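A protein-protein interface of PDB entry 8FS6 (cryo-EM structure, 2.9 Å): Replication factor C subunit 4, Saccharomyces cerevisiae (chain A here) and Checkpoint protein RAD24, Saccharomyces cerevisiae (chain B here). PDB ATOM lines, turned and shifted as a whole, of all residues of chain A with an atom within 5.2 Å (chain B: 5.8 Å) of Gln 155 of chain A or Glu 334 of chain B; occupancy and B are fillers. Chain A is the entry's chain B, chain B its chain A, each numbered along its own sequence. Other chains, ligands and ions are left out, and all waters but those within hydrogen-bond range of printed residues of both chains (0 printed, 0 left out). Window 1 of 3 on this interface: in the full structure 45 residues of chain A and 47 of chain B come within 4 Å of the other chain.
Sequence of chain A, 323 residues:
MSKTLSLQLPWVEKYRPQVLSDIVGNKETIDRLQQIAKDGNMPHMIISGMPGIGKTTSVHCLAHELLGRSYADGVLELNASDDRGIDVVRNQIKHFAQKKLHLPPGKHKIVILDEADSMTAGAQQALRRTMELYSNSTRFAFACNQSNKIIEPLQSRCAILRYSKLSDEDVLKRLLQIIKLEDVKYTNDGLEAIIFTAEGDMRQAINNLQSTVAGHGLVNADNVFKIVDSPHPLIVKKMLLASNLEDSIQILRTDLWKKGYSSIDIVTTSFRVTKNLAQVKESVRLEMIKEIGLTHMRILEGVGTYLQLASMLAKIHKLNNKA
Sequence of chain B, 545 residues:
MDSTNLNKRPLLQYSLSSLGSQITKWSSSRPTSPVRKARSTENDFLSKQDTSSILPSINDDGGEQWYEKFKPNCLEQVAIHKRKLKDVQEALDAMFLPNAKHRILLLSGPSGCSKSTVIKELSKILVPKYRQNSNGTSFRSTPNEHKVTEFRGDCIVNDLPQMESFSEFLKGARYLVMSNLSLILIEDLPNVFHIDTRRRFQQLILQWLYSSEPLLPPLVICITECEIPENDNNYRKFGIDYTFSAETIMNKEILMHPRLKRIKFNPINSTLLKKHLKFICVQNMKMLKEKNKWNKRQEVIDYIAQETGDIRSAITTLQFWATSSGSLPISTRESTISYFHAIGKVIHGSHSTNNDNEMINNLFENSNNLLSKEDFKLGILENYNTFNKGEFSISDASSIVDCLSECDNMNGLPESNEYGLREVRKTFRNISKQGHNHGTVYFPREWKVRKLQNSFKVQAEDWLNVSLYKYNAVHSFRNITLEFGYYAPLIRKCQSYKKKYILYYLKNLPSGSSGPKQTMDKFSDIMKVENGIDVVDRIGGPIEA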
ATOM      1  N   ILE A  46     -26.029  22.540 -31.759  1.00  0.00           N
ATOM      2  CA  ILE A  46     -25.140  21.418 -31.491  1.00  0.00           C
ATOM      3  C   ILE A  46     -25.319  20.430 -32.635  1.00  0.00           C
ATOM      4  O   ILE A  46     -26.396  19.841 -32.792  1.00  0.00           O
ATOM      5  CB  ILE A  46     -25.434  20.756 -30.138  1.00  0.00           C
ATOM      6  CG1 ILE A  46     -25.099  21.712 -28.991  1.00  0.00           C
ATOM      7  CG2 ILE A  46     -24.656  19.458 -29.999  1.00  0.00           C
ATOM      8  CD1 ILE A  46     -25.266  21.100 -27.617  1.00  0.00           C
ATOM      9  N   SER A 147     -23.740  13.630 -28.317  1.00  0.00           N
ATOM     10  CA  SER A 147     -24.394  14.774 -27.691  1.00  0.00           C
ATOM     11  C   SER A 147     -24.426  14.677 -26.172  1.00  0.00           C
ATOM     12  O   SER A 147     -24.501  15.713 -25.502  1.00  0.00           O
ATOM     13  CB  SER A 147     -25.818  14.925 -28.225  1.00  0.00           C
ATOM     14  OG  SER A 147     -25.819  15.452 -29.540  1.00  0.00           O
ATOM     15  N   ASN A 148     -24.373  13.468 -25.611  1.00  0.00           N
ATOM     16  CA  ASN A 148     -24.447  13.311 -24.163  1.00  0.00           C
ATOM     17  C   ASN A 148     -23.179  13.760 -23.448  1.00  0.00           C
ATOM     18  O   ASN A 148     -23.191  13.864 -22.217  1.00  0.00           O
ATOM     19  CB  ASN A 148     -24.754  11.857 -23.801  1.00  0.00           C
ATOM     20  CG  ASN A 148     -24.023  10.869 -24.685  1.00  0.00           C
ATOM     21  OD1 ASN A 148     -24.541  10.436 -25.716  1.00  0.00           O
ATOM     22  ND2 ASN A 148     -22.804  10.517 -24.294  1.00  0.00           N
ATOM     23  N   ILE A 150     -21.912  16.708 -23.725  1.00  0.00           N
ATOM     24  CA  ILE A 150     -22.116  18.111 -23.385  1.00  0.00           C
ATOM     25  C   ILE A 150     -23.155  18.173 -22.276  1.00  0.00           C
ATOM     26  O   ILE A 150     -24.196  17.509 -22.356  1.00  0.00           O
ATOM     27  CB  ILE A 150     -22.553  18.926 -24.614  1.00  0.00           C
ATOM     28  CG1 ILE A 150     -21.380  19.091 -25.581  1.00  0.00           C
ATOM     29  CG2 ILE A 150     -23.086  20.286 -24.206  1.00  0.00           C
ATOM     30  CD1 ILE A 150     -21.619  18.475 -26.929  1.00  0.00           C
ATOM     31  N   ILE A 151     -22.864  18.955 -21.231  1.00  0.00           N
ATOM     32  CA  ILE A 151     -23.716  18.971 -20.050  1.00  0.00           C
ATOM     33  C   ILE A 151     -25.121  19.452 -20.404  1.00  0.00           C
ATOM     34  O   ILE A 151     -25.326  20.221 -21.352  1.00  0.00           O
ATOM     35  CB  ILE A 151     -23.099  19.842 -18.943  1.00  0.00           C
ATOM     36  CG1 ILE A 151     -22.883  21.271 -19.440  1.00  0.00           C
ATOM     37  CG2 ILE A 151     -21.788  19.239 -18.459  1.00  0.00           C
ATOM     38  CD1 ILE A 151     -22.645  22.273 -18.332  1.00  0.00           C
ATOM     39  N   GLU A 152     -26.099  18.973 -19.634  1.00  0.00           N
ATOM     40  CA  GLU A 152     -27.497  19.304 -19.896  1.00  0.00           C
ATOM     41  C   GLU A 152     -27.807  20.800 -19.868  1.00  0.00           C
ATOM     42  O   GLU A 152     -28.578  21.249 -20.736  1.00  0.00           O
ATOM     43  CB  GLU A 152     -28.393  18.544 -18.909  1.00  0.00           C
ATOM     44  CG  GLU A 152     -27.970  17.103 -18.682  1.00  0.00           C
ATOM     45  CD  GLU A 152     -28.754  16.128 -19.534  1.00  0.00           C
ATOM     46  OE1 GLU A 152     -29.928  16.423 -19.841  1.00  0.00           O
ATOM     47  OE2 GLU A 152     -28.197  15.071 -19.901  1.00  0.00           O
ATOM     48  N   PRO A 153     -27.300  21.609 -18.926  1.00  0.00           N
ATOM     49  CA  PRO A 153     -27.556  23.057 -19.011  1.00  0.00           C
ATOM     50  C   PRO A 153     -27.030  23.698 -20.283  1.00  0.00           C
ATOM     51  O   PRO A 153     -27.628  24.672 -20.759  1.00  0.00           O
ATOM     52  CB  PRO A 153     -26.847  23.612 -17.771  1.00  0.00           C
ATOM     53  CG  PRO A 153     -26.846  22.486 -16.819  1.00  0.00           C
ATOM     54  CD  PRO A 153     -26.614  21.273 -17.663  1.00  0.00           C
ATOM     55  N   LEU A 154     -25.932  23.193 -20.849  1.00  0.00           N
ATOM     56  CA  LEU A 154     -25.453  23.712 -22.124  1.00  0.00           C
ATOM     57  C   LEU A 154     -26.329  23.259 -23.284  1.00  0.00           C
ATOM     58  O   LEU A 154     -26.551  24.029 -24.225  1.00  0.00           O
ATOM     59  CB  LEU A 154     -24.009  23.276 -22.369  1.00  0.00           C
ATOM     60  CG  LEU A 154     -22.901  24.129 -21.748  1.00  0.00           C
ATOM     61  CD1 LEU A 154     -21.562  23.818 -22.398  1.00  0.00           C
ATOM     62  CD2 LEU A 154     -23.226  25.605 -21.838  1.00  0.00           C
ATOM     63  N   GLN A 155     -26.823  22.019 -23.239  1.00  0.00           N
ATOM     64  CA  GLN A 155     -27.726  21.530 -24.275  1.00  0.00           C
ATOM     65  C   GLN A 155     -29.084  22.214 -24.224  1.00  0.00           C
ATOM     66  O   GLN A 155     -29.785  22.247 -25.241  1.00  0.00           O
ATOM     67  CB  GLN A 155     -27.907  20.018 -24.143  1.00  0.00           C
ATOM     68  CG  GLN A 155     -26.687  19.202 -24.534  1.00  0.00           C
ATOM     69  CD  GLN A 155     -27.002  17.727 -24.686  1.00  0.00           C
ATOM     70  OE1 GLN A 155     -27.669  17.317 -25.636  1.00  0.00           O
ATOM     71  NE2 GLN A 155     -26.523  16.920 -23.747  1.00  0.00           N
ATOM     72  N   SER A 156     -29.473  22.745 -23.062  1.00  0.00           N
ATOM     73  CA  SER A 156     -30.770  23.402 -22.938  1.00  0.00           C
ATOM     74  C   SER A 156     -30.843  24.664 -23.791  1.00  0.00           C
ATOM     75  O   SER A 156     -31.869  24.929 -24.428  1.00  0.00           O
ATOM     76  CB  SER A 156     -31.049  23.730 -21.471  1.00  0.00           C
ATOM     77  OG  SER A 156     -32.151  24.610 -21.346  1.00  0.00           O
ATOM     78  N   ARG A 157     -29.769  25.453 -23.816  1.00  0.00           N
ATOM     79  CA  ARG A 157     -29.766  26.715 -24.544  1.00  0.00           C
ATOM     80  C   ARG A 157     -29.502  26.550 -26.034  1.00  0.00           C
ATOM     81  O   ARG A 157     -29.583  27.538 -26.772  1.00  0.00           O
ATOM     82  CB  ARG A 157     -28.720  27.661 -23.948  1.00  0.00           C
ATOM     83  CG  ARG A 157     -28.783  27.786 -22.436  1.00  0.00           C
ATOM     84  CD  ARG A 157     -27.465  28.288 -21.872  1.00  0.00           C
ATOM     85  NE  ARG A 157     -27.443  28.246 -20.415  1.00  0.00           N
ATOM     86  CZ  ARG A 157     -27.878  29.224 -19.631  1.00  0.00           C
ATOM     87  NH1 ARG A 157     -28.376  30.342 -20.132  1.00  0.00           N
ATOM     88  NH2 ARG A 157     -27.809  29.075 -18.311  1.00  0.00           N
ATOM     89  N   CYS A 158     -29.193  25.342 -26.492  1.00  0.00           N
ATOM     90  CA  CYS A 158     -28.835  25.104 -27.883  1.00  0.00           C
ATOM     91  C   CYS A 158     -29.973  24.413 -28.628  1.00  0.00           C
ATOM     92  O   CYS A 158     -30.937  23.919 -28.038  1.00  0.00           O
ATOM     93  CB  CYS A 158     -27.558  24.264 -27.969  1.00  0.00           C
ATOM     94  SG  CYS A 158     -26.052  25.146 -27.501  1.00  0.00           S
ATOM     95  N   ALA A 159     -29.848  24.392 -29.953  1.00  0.00           N
ATOM     96  CA  ALA A 159     -30.762  23.672 -30.831  1.00  0.00           C
ATOM     97  C   ALA A 159     -30.025  22.465 -31.391  1.00  0.00           C
ATOM     98  O   ALA A 159     -28.990  22.617 -32.048  1.00  0.00           O
ATOM     99  CB  ALA A 159     -31.271  24.571 -31.959  1.00  0.00           C
ATOM    100  N   ILE A 160     -30.556  21.275 -31.139  1.00  0.00           N
ATOM    101  CA  ILE A 160     -29.852  20.042 -31.473  1.00  0.00           C
ATOM    102  C   ILE A 160     -30.112  19.699 -32.936  1.00  0.00           C
ATOM    103  O   ILE A 160     -31.265  19.554 -33.358  1.00  0.00           O
ATOM    104  CB  ILE A 160     -30.277  18.893 -30.547  1.00  0.00           C
ATOM    105  CG1 ILE A 160     -29.648  19.062 -29.161  1.00  0.00           C
ATOM    106  CG2 ILE A 160     -29.868  17.557 -31.132  1.00  0.00           C
ATOM    107  CD1 ILE A 160     -30.493  19.858 -28.186  1.00  0.00           C
ATOM    108  N   ARG A 162     -29.141  16.809 -35.487  1.00  0.00           N
ATOM    109  CA  ARG A 162     -28.587  15.457 -35.518  1.00  0.00           C
ATOM    110  C   ARG A 162     -28.302  15.063 -36.962  1.00  0.00           C
ATOM    111  O   ARG A 162     -29.216  14.735 -37.723  1.00  0.00           O
ATOM    112  CB  ARG A 162     -29.538  14.471 -34.850  1.00  0.00           C
ATOM    113  CG  ARG A 162     -29.753  14.746 -33.378  1.00  0.00           C
ATOM    114  CD  ARG A 162     -30.773  13.806 -32.765  1.00  0.00           C
ATOM    115  NE  ARG A 162     -31.103  14.196 -31.399  1.00  0.00           N
ATOM    116  CZ  ARG A 162     -30.346  13.940 -30.341  1.00  0.00           C
ATOM    117  NH1 ARG A 162     -29.208  13.276 -30.450  1.00  0.00           N
ATOM    118  NH2 ARG A 162     -30.742  14.361 -29.143  1.00  0.00           N
ATOM    119  N   GLU B 307     -42.175  15.161 -25.019  1.00  0.00           N
ATOM    120  CA  GLU B 307     -40.768  14.784 -25.079  1.00  0.00           C
ATOM    121  C   GLU B 307     -39.937  15.362 -23.944  1.00  0.00           C
ATOM    122  O   GLU B 307     -39.176  14.622 -23.322  1.00  0.00           O
ATOM    123  CB  GLU B 307     -40.144  15.231 -26.410  1.00  0.00           C
ATOM    124  CG  GLU B 307     -38.589  15.301 -26.489  1.00  0.00           C
ATOM    125  CD  GLU B 307     -37.807  14.026 -26.115  1.00  0.00           C
ATOM    126  OE1 GLU B 307     -36.639  13.952 -26.542  1.00  0.00           O
ATOM    127  OE2 GLU B 307     -38.330  13.074 -25.497  1.00  0.00           O
ATOM    128  N   SER B 313     -35.416  24.697 -23.601  1.00  0.00           N
ATOM    129  CA  SER B 313     -35.245  23.879 -24.794  1.00  0.00           C
ATOM    130  C   SER B 313     -36.533  23.731 -25.592  1.00  0.00           C
ATOM    131  O   SER B 313     -36.470  23.659 -26.821  1.00  0.00           O
ATOM    132  CB  SER B 313     -34.707  22.498 -24.416  1.00  0.00           C
ATOM    133  OG  SER B 313     -34.250  21.801 -25.561  1.00  0.00           O
ATOM    134  N   THR B 332     -35.088  17.594 -29.376  1.00  0.00           N
ATOM    135  CA  THR B 332     -34.933  18.260 -28.093  1.00  0.00           C
ATOM    136  C   THR B 332     -33.809  17.563 -27.336  1.00  0.00           C
ATOM    137  O   THR B 332     -33.403  16.450 -27.680  1.00  0.00           O
ATOM    138  CB  THR B 332     -36.248  18.241 -27.297  1.00  0.00           C
ATOM    139  OG1 THR B 332     -37.344  18.485 -28.185  1.00  0.00           O
ATOM    140  CG2 THR B 332     -36.257  19.330 -26.238  1.00  0.00           C
ATOM    141  N   ARG B 333     -33.292  18.235 -26.308  1.00  0.00           N
ATOM    142  CA  ARG B 333     -32.209  17.671 -25.514  1.00  0.00           C
ATOM    143  C   ARG B 333     -32.663  16.394 -24.815  1.00  0.00           C
ATOM    144  O   ARG B 333     -33.835  16.231 -24.458  1.00  0.00           O
ATOM    145  CB  ARG B 333     -31.705  18.696 -24.492  1.00  0.00           C
ATOM    146  CG  ARG B 333     -32.440  18.695 -23.159  1.00  0.00           C
ATOM    147  CD  ARG B 333     -31.684  19.479 -22.100  1.00  0.00           C
ATOM    148  NE  ARG B 333     -32.503  19.724 -20.919  1.00  0.00           N
ATOM    149  CZ  ARG B 333     -32.603  18.892 -19.891  1.00  0.00           C
ATOM    150  NH1 ARG B 333     -31.945  17.745 -19.864  1.00  0.00           N
ATOM    151  NH2 ARG B 333     -33.385  19.219 -18.866  1.00  0.00           N
ATOM    152  N   GLU B 334     -31.727  15.464 -24.656  1.00  0.00           N
ATOM    153  CA  GLU B 334     -32.026  14.184 -24.035  1.00  0.00           C
ATOM    154  C   GLU B 334     -31.926  14.284 -22.519  1.00  0.00           C
ATOM    155  O   GLU B 334     -31.110  15.034 -21.976  1.00  0.00           O
ATOM    156  CB  GLU B 334     -31.075  13.102 -24.547  1.00  0.00           C
ATOM    157  CG  GLU B 334     -30.659  13.279 -25.996  1.00  0.00           C
ATOM    158  CD  GLU B 334     -29.305  13.943 -26.137  1.00  0.00           C
ATOM    159  OE1 GLU B 334     -28.671  14.234 -25.101  1.00  0.00           O
ATOM    160  OE2 GLU B 334     -28.874  14.178 -27.287  1.00  0.00           O
ATOM    161  N   SER B 335     -32.767  13.516 -21.837  1.00  0.00           N
ATOM    162  CA  SER B 335     -32.778  13.465 -20.384  1.00  0.00           C
ATOM    163  C   SER B 335     -31.958  12.279 -19.896  1.00  0.00           C
ATOM    164  O   SER B 335     -31.916  11.223 -20.532  1.00  0.00           O
ATOM    165  CB  SER B 335     -34.209  13.366 -19.851  1.00  0.00           C
ATOM    166  OG  SER B 335     -35.085  14.208 -20.581  1.00  0.00           O
ATOM    167  N   THR B 336     -31.301  12.465 -18.755  1.00  0.00           N
ATOM    168  CA  THR B 336     -30.460  11.437 -18.156  1.00  0.00           C
ATOM    169  C   THR B 336     -31.304  10.601 -17.203  1.00  0.00           C
ATOM    170  O   THR B 336     -31.890  11.134 -16.254  1.00  0.00           O
ATOM    171  CB  THR B 336     -29.272  12.058 -17.421  1.00  0.00           C
ATOM    172  OG1 THR B 336     -28.348  12.598 -18.375  1.00  0.00           O
ATOM    173  CG2 THR B 336     -28.560  11.010 -16.577  1.00  0.00           C
ATOM    174  N   ASN B 366     -26.687   5.885 -23.346  1.00  0.00           N
ATOM    175  CA  ASN B 366     -27.115   7.187 -22.849  1.00  0.00           C
ATOM    176  C   ASN B 366     -26.750   7.377 -21.382  1.00  0.00           C
ATOM    177  O   ASN B 366     -26.596   8.512 -20.918  1.00  0.00           O
ATOM    178  CB  ASN B 366     -28.622   7.361 -23.044  1.00  0.00           C
ATOM    179  CG  ASN B 366     -28.967   8.014 -24.368  1.00  0.00           C
ATOM    180  OD1 ASN B 366     -28.186   8.798 -24.908  1.00  0.00           O
ATOM    181  ND2 ASN B 366     -30.143   7.696 -24.896  1.00  0.00           N
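The guanidinium group of Arg 333 of chain B lies within salt-bridge range of the side-chain carboxylate of Glu 152 of chain A, 2.4 Å away.
The side-chain amide oxygen of Gln 155 of chain A sits close to the side-chain carboxylate of Glu 334 of chain B (3.3 Å).
NH2 of Arg 162 of chain A is in salt-bridge range of OE2 of Glu 334 of chain B, 2.6 Å away.
OE2 of Glu 152 of chain A is in hydrogen-bond range of OG1 of Thr 336 of chain B (2.9 Å).
The side-chain carboxylate (OE1) of Glu 152 of chain A sits close to the backbone carbonyl oxygen (O) of Glu 334 of chain B (2.8 Å).
Among the printed residues, merely in contact across the chains: Ser 147 of chain A with Glu 334 of chain B, Ser 156 of chain A with Ser 313 of chain B, Ile 160 of chain A with Arg 333 of chain B and Arg 162 of chain A with Thr 332 of chain B.
O of Ser 147 of chain A lies within hydrogen-bond range of NE2 of Gln 155 of chain A, at 2.9 Å.
O of Ile 150 of chain A is in hydrogen-bond range of NE2 of Gln 155 of chain A (2.8 Å).
Along chain B the printed residues that touch a printed residue of chain A span positions 313 to 336.
Of the 15 printed residues of chain A, 6 touch a printed residue of chain B.
Printed residues of chain A that touch a printed residue of chain B: Ser 147, Glu 152, Gln 155, Ser 156, Ile 160 and Arg 162.
Of the printed residues of chain B, Gln 155 of chain A touches Glu 334 (3.3 Å).
Of the printed residues of chain A, Arg 333 of chain B touches Glu 152 and Ile 160.
Of the printed residues of chain B, Arg 162 of chain A touches Thr 332 and Glu 334.
The nearest residue of chain A that does not touch Glu 334 of chain B is Asn 148 of chain A (4.4 Å).
The nearest printed residue of chain A that does not touch Arg 333 of chain B is Gln 155 of chain A (4.04 Å).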
